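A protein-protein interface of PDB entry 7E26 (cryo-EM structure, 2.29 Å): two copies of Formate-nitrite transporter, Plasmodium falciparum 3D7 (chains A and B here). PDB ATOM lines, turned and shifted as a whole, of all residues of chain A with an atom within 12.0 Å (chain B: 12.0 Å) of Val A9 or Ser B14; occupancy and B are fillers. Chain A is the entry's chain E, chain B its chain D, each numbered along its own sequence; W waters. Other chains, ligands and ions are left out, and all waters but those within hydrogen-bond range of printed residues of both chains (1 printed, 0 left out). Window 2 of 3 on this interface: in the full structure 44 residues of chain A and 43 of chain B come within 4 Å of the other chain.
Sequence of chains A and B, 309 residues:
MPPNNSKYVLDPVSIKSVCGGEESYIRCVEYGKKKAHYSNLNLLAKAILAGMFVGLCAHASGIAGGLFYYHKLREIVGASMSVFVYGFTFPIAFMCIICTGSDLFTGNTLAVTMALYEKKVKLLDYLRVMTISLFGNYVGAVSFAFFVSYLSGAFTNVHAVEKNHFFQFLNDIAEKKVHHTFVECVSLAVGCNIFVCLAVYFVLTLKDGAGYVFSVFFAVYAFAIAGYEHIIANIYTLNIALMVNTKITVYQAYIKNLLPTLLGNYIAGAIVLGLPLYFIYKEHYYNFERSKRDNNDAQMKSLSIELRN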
ATOM      1  N   LYS A   7      19.310  -7.364 -22.282  1.00  0.00           N
ATOM      2  CA  LYS A   7      19.322  -8.818 -22.368  1.00  0.00           C
ATOM      3  C   LYS A   7      20.450  -9.403 -21.531  1.00  0.00           C
ATOM      4  O   LYS A   7      21.624  -9.193 -21.823  1.00  0.00           O
ATOM      5  CB  LYS A   7      19.458  -9.270 -23.821  1.00  0.00           C
ATOM      6  N   TYR A   8      20.086 -10.142 -20.490  1.00  0.00           N
ATOM      7  CA  TYR A   8      21.041 -10.721 -19.557  1.00  0.00           C
ATOM      8  C   TYR A   8      21.022 -12.234 -19.692  1.00  0.00           C
ATOM      9  O   TYR A   8      19.949 -12.840 -19.769  1.00  0.00           O
ATOM     10  CB  TYR A   8      20.718 -10.310 -18.117  1.00  0.00           C
ATOM     11  CG  TYR A   8      20.424  -8.836 -17.949  1.00  0.00           C
ATOM     12  CD1 TYR A   8      21.455  -7.912 -17.835  1.00  0.00           C
ATOM     13  CD2 TYR A   8      19.117  -8.370 -17.908  1.00  0.00           C
ATOM     14  CE1 TYR A   8      21.190  -6.567 -17.686  1.00  0.00           C
ATOM     15  CE2 TYR A   8      18.846  -7.028 -17.760  1.00  0.00           C
ATOM     16  CZ  TYR A   8      19.884  -6.133 -17.649  1.00  0.00           C
ATOM     17  OH  TYR A   8      19.613  -4.797 -17.501  1.00  0.00           O
ATOM     18  N   VAL A   9      22.203 -12.838 -19.723  1.00  0.00           N
ATOM     19  CA  VAL A   9      22.337 -14.287 -19.803  1.00  0.00           C
ATOM     20  C   VAL A   9      22.514 -14.816 -18.385  1.00  0.00           C
ATOM     21  O   VAL A   9      23.516 -14.530 -17.726  1.00  0.00           O
ATOM     22  CB  VAL A   9      23.507 -14.698 -20.702  1.00  0.00           C
ATOM     23  CG1 VAL A   9      23.716 -16.194 -20.644  1.00  0.00           C
ATOM     24  CG2 VAL A   9      23.255 -14.254 -22.127  1.00  0.00           C
ATOM     25  N   LEU A  10      21.565 -15.591 -17.909  1.00  0.00           N
ATOM     26  CA  LEU A  10      21.655 -16.152 -16.601  1.00  0.00           C
ATOM     27  C   LEU A  10      22.264 -17.516 -16.722  1.00  0.00           C
ATOM     28  O   LEU A  10      23.224 -17.762 -16.076  1.00  0.00           O
ATOM     29  CB  LEU A  10      20.287 -16.213 -15.947  1.00  0.00           C
ATOM     30  CG  LEU A  10      20.009 -15.236 -14.810  1.00  0.00           C
ATOM     31  CD1 LEU A  10      20.637 -15.703 -13.521  1.00  0.00           C
ATOM     32  CD2 LEU A  10      20.575 -13.888 -15.184  1.00  0.00           C
ATOM     33  N   ASP A  11      21.707 -18.405 -17.546  1.00  0.00           N
ATOM     34  CA  ASP A  11      22.243 -19.749 -17.733  1.00  0.00           C
ATOM     35  C   ASP A  11      22.757 -19.877 -19.157  1.00  0.00           C
ATOM     36  O   ASP A  11      21.952 -19.861 -20.108  1.00  0.00           O
ATOM     37  CB  ASP A  11      21.184 -20.809 -17.443  1.00  0.00           C
ATOM     38  CG  ASP A  11      21.783 -22.098 -16.923  1.00  0.00           C
ATOM     39  OD1 ASP A  11      22.720 -22.029 -16.102  1.00  0.00           O
ATOM     40  OD2 ASP A  11      21.322 -23.181 -17.338  1.00  0.00           O
ATOM     41  N   PRO A  12      24.059 -19.985 -19.362  1.00  0.00           N
ATOM     42  CA  PRO A  12      24.603 -20.129 -20.710  1.00  0.00           C
ATOM     43  C   PRO A  12      24.495 -21.568 -21.207  1.00  0.00           C
ATOM     44  O   PRO A  12      23.951 -22.446 -20.544  1.00  0.00           O
ATOM     45  CB  PRO A  12      26.060 -19.702 -20.541  1.00  0.00           C
ATOM     46  CG  PRO A  12      26.183 -19.136 -19.172  1.00  0.00           C
ATOM     47  CD  PRO A  12      25.118 -19.765 -18.367  1.00  0.00           C
ATOM     48  N   VAL A  13      25.034 -21.796 -22.400  1.00  0.00           N
ATOM     49  CA  VAL A  13      24.961 -23.099 -23.052  1.00  0.00           C
ATOM     50  C   VAL A  13      26.033 -24.008 -22.471  1.00  0.00           C
ATOM     51  O   VAL A  13      27.211 -23.644 -22.413  1.00  0.00           O
ATOM     52  CB  VAL A  13      25.114 -22.949 -24.574  1.00  0.00           C
ATOM     53  CG1 VAL A  13      25.196 -24.299 -25.252  1.00  0.00           C
ATOM     54  CG2 VAL A  13      23.961 -22.156 -25.136  1.00  0.00           C
ATOM     55  N   SER A  14      25.628 -25.197 -22.039  1.00  0.00           N
ATOM     56  CA  SER A  14      26.545 -26.140 -21.415  1.00  0.00           C
ATOM     57  C   SER A  14      27.360 -26.855 -22.488  1.00  0.00           C
ATOM     58  O   SER A  14      26.795 -27.500 -23.375  1.00  0.00           O
ATOM     59  CB  SER A  14      25.763 -27.132 -20.562  1.00  0.00           C
ATOM     60  OG  SER A  14      26.629 -28.014 -19.883  1.00  0.00           O
ATOM     61  N   ILE A  15      28.685 -26.735 -22.409  1.00  0.00           N
ATOM     62  CA  ILE A  15      29.595 -27.349 -23.370  1.00  0.00           C
ATOM     63  C   ILE A  15      30.548 -28.297 -22.658  1.00  0.00           C
ATOM     64  O   ILE A  15      30.524 -28.415 -21.429  1.00  0.00           O
ATOM     65  CB  ILE A  15      30.430 -26.309 -24.123  1.00  0.00           C
ATOM     66  CG1 ILE A  15      31.223 -25.534 -23.084  1.00  0.00           C
ATOM     67  CG2 ILE A  15      29.548 -25.422 -24.971  1.00  0.00           C
ATOM     68  CD1 ILE A  15      32.633 -25.381 -23.403  1.00  0.00           C
ATOM     69  N   LYS A  16      31.421 -28.937 -23.430  1.00  0.00           N
ATOM     70  CA  LYS A  16      32.348 -29.935 -22.916  1.00  0.00           C
ATOM     71  C   LYS A  16      33.466 -30.114 -23.929  1.00  0.00           C
ATOM     72  O   LYS A  16      33.195 -30.329 -25.110  1.00  0.00           O
ATOM     73  CB  LYS A  16      31.616 -31.254 -22.660  1.00  0.00           C
ATOM     74  CG  LYS A  16      32.466 -32.481 -22.698  1.00  0.00           C
ATOM     75  CD  LYS A  16      31.614 -33.713 -22.802  1.00  0.00           C
ATOM     76  CE  LYS A  16      30.831 -33.729 -24.084  1.00  0.00           C
ATOM     77  NZ  LYS A  16      30.157 -35.030 -24.268  1.00  0.00           N
ATOM     78  N   VAL B   9      32.784  -9.482 -34.855  1.00  0.00           N
ATOM     79  CA  VAL B   9      32.030 -10.061 -33.750  1.00  0.00           C
ATOM     80  C   VAL B   9      32.253  -9.182 -32.526  1.00  0.00           C
ATOM     81  O   VAL B   9      33.369  -9.085 -32.013  1.00  0.00           O
ATOM     82  CB  VAL B   9      32.448 -11.509 -33.480  1.00  0.00           C
ATOM     83  CG1 VAL B   9      31.762 -12.030 -32.238  1.00  0.00           C
ATOM     84  CG2 VAL B   9      32.117 -12.382 -34.672  1.00  0.00           C
ATOM     85  N   LEU B  10      31.188  -8.532 -32.064  1.00  0.00           N
ATOM     86  CA  LEU B  10      31.255  -7.687 -30.878  1.00  0.00           C
ATOM     87  C   LEU B  10      30.880  -8.445 -29.618  1.00  0.00           C
ATOM     88  O   LEU B  10      31.577  -8.344 -28.604  1.00  0.00           O
ATOM     89  CB  LEU B  10      30.344  -6.467 -31.037  1.00  0.00           C
ATOM     90  CG  LEU B  10      30.954  -5.156 -31.533  1.00  0.00           C
ATOM     91  CD1 LEU B  10      31.842  -4.566 -30.458  1.00  0.00           C
ATOM     92  CD2 LEU B  10      31.750  -5.363 -32.807  1.00  0.00           C
ATOM     93  N   ASP B  11      29.794  -9.200 -29.664  1.00  0.00           N
ATOM     94  CA  ASP B  11      29.380 -10.039 -28.544  1.00  0.00           C
ATOM     95  C   ASP B  11      29.310 -11.481 -29.015  1.00  0.00           C
ATOM     96  O   ASP B  11      28.440 -11.821 -29.838  1.00  0.00           O
ATOM     97  CB  ASP B  11      28.034  -9.587 -27.985  1.00  0.00           C
ATOM     98  CG  ASP B  11      27.895  -9.877 -26.507  1.00  0.00           C
ATOM     99  OD1 ASP B  11      28.883  -9.683 -25.768  1.00  0.00           O
ATOM    100  OD2 ASP B  11      26.803 -10.305 -26.082  1.00  0.00           O
ATOM    101  N   PRO B  12      30.194 -12.350 -28.553  1.00  0.00           N
ATOM    102  CA  PRO B  12      30.159 -13.754 -28.961  1.00  0.00           C
ATOM    103  C   PRO B  12      29.110 -14.538 -28.177  1.00  0.00           C
ATOM    104  O   PRO B  12      28.368 -13.997 -27.364  1.00  0.00           O
ATOM    105  CB  PRO B  12      31.573 -14.239 -28.645  1.00  0.00           C
ATOM    106  CG  PRO B  12      32.370 -13.034 -28.296  1.00  0.00           C
ATOM    107  CD  PRO B  12      31.409 -12.035 -27.790  1.00  0.00           C
ATOM    108  N   VAL B  13      29.067 -15.839 -28.439  1.00  0.00           N
ATOM    109  CA  VAL B  13      28.079 -16.724 -27.828  1.00  0.00           C
ATOM    110  C   VAL B  13      28.540 -17.093 -26.426  1.00  0.00           C
ATOM    111  O   VAL B  13      29.672 -17.542 -26.229  1.00  0.00           O
ATOM    112  CB  VAL B  13      27.865 -17.974 -28.698  1.00  0.00           C
ATOM    113  CG1 VAL B  13      26.963 -18.975 -28.007  1.00  0.00           C
ATOM    114  CG2 VAL B  13      27.279 -17.584 -30.032  1.00  0.00           C
ATOM    115  N   SER B  14      27.663 -16.905 -25.448  1.00  0.00           N
ATOM    116  CA  SER B  14      27.996 -17.169 -24.056  1.00  0.00           C
ATOM    117  C   SER B  14      27.916 -18.667 -23.781  1.00  0.00           C
ATOM    118  O   SER B  14      26.866 -19.285 -23.980  1.00  0.00           O
ATOM    119  CB  SER B  14      27.057 -16.390 -23.143  1.00  0.00           C
ATOM    120  OG  SER B  14      27.402 -16.566 -21.788  1.00  0.00           O
ATOM    121  N   ILE B  15      29.026 -19.252 -23.331  1.00  0.00           N
ATOM    122  CA  ILE B  15      29.110 -20.679 -23.039  1.00  0.00           C
ATOM    123  C   ILE B  15      29.491 -20.892 -21.583  1.00  0.00           C
ATOM    124  O   ILE B  15      29.743 -19.935 -20.845  1.00  0.00           O
ATOM    125  CB  ILE B  15      30.144 -21.392 -23.915  1.00  0.00           C
ATOM    126  CG1 ILE B  15      31.487 -20.731 -23.648  1.00  0.00           C
ATOM    127  CG2 ILE B  15      29.742 -21.341 -25.371  1.00  0.00           C
ATOM    128  CD1 ILE B  15      32.572 -21.667 -23.404  1.00  0.00           C
ATOM    129  N   LYS B  16      29.582 -22.158 -21.182  1.00  0.00           N
ATOM    130  CA  LYS B  16      29.863 -22.532 -19.804  1.00  0.00           C
ATOM    131  C   LYS B  16      30.341 -23.974 -19.789  1.00  0.00           C
ATOM    132  O   LYS B  16      29.685 -24.845 -20.359  1.00  0.00           O
ATOM    133  CB  LYS B  16      28.610 -22.357 -18.943  1.00  0.00           C
ATOM    134  CG  LYS B  16      28.546 -23.204 -17.716  1.00  0.00           C
ATOM    135  CD  LYS B  16      27.152 -23.227 -17.158  1.00  0.00           C
ATOM    136  CE  LYS B  16      26.189 -23.851 -18.125  1.00  0.00           C
ATOM    137  NZ  LYS B  16      24.868 -24.052 -17.492  1.00  0.00           N
ATOM    138  N   SER B  17      31.488 -24.225 -19.161  1.00  0.00           N
ATOM    139  CA  SER B  17      32.035 -25.574 -19.092  1.00  0.00           C
ATOM    140  C   SER B  17      31.963 -26.158 -17.689  1.00  0.00           C
ATOM    141  O   SER B  17      32.745 -27.050 -17.356  1.00  0.00           O
ATOM    142  CB  SER B  17      33.477 -25.594 -19.592  1.00  0.00           C
ATOM    143  OG  SER B  17      34.383 -25.341 -18.537  1.00  0.00           O
ATOM    144  N   VAL B  18      31.054 -25.656 -16.855  1.00  0.00           N
ATOM    145  CA  VAL B  18      30.907 -26.087 -15.473  1.00  0.00           C
ATOM    146  C   VAL B  18      29.443 -26.456 -15.238  1.00  0.00           C
ATOM    147  O   VAL B  18      28.582 -26.227 -16.083  1.00  0.00           O
ATOM    148  CB  VAL B  18      31.376 -25.008 -14.476  1.00  0.00           C
ATOM    149  CG1 VAL B  18      32.868 -24.754 -14.623  1.00  0.00           C
ATOM    150  CG2 VAL B  18      30.606 -23.725 -14.679  1.00  0.00           C
HETATM  151  O   HOH W   1      26.049 -28.155 -17.072  1.00  0.00           O
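N of Ile A15 lies within hydrogen-bond range of O of Lys B16, 3.0 Å away.
O of Val A13 is in hydrogen-bond range of N of Lys B16 (3.1 Å).
NZ of Lys B16 lies within salt-bridge range of OD1 of Asp A11, at 3.3 Å.
The backbone NH of Val A13 lies within hydrogen-bond range of the backbone carbonyl oxygen of Ser B14, 3.5 Å away.
Among the printed residues, pairs that only touch across the chains: Val A9 with Ser B14 (3.9 Å), Pro A12 with Ser B14 (3.6 Å), Pro A12 with Ile B15 (3.7 Å), Pro A12 with Lys B16 (3.6 Å), Val A13 with Ile B15 (3.6 Å), Ser A14 with Lys B16 (3.6 Å), Ile A15 with Ile B15 (3.7 Å) and Ile A15 with Ser B17 (3.9 Å).
No residue of chain B comes within 4 Å of Lys A7.
Val A9 touches just one residue of chain B: Ser B14 (3.9 Å).
No residue of chain B comes within 4 Å of Leu A10.
Printed residues of chain B within 4 Å of Asp A11: Lys B16 (3.3 Å).
Pro A12 touches just these residues of chain B: Ser B14, Ile B15 and Lys B16.
Val A13 touches three residues of chain B.
Of the printed residues of chain B, Ile A15 touches Ile B15, Lys B16 and Ser B17.
Pro B12 touches none of the printed residues of chain A.
No residue of chain A comes within 4 Å of Val B13.
Of chain A, only Val A9, Pro A12 and Val A13 come within 4 Å of Ser B14.
Of the printed residues of chain A, Lys B16 touches Asp A11, Pro A12, Val A13, Ser A14 and Ile A15.
Printed residues of chain A within 4 Å of Ser B17: Ile A15 (3.9 Å).
The nearest residue of chain A that does not touch Ser B14 is Asp A11 (6.3 Å).
Printed residues of chain A that touch a printed residue of chain B: Val A9, Asp A11, Pro A12, Val A13, Ser A14 and Ile A15.
Of the 10 printed residues of chain B, 4 touch a printed residue of chain A.
Among the printed residues, Asp or Glu carboxylates within 4 Å of a Lys or Arg side-chain nitrogen of the other chain: Asp A11 with Lys B16 (3.3 Å).
Val A9 touches Ser B14, but with the chains exchanged Ser A14 does not touch Val B9 (17.7 Å).
Asp A11 touches Lys B16, but with the chains exchanged Lys A16 does not touch Asp B11 (18.4 Å).
Pro A12 touches Ile B15, but with the chains exchanged Ile A15 does not touch Pro B12 (11.4 Å).
Ile A15 touches Lys B16, but with the chains exchanged Lys A16 does not touch Ile B15 (7.4 Å).
8 positions are printed for both chains.
Water W1 bridges OG of Ser A14 and O of Val B18.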
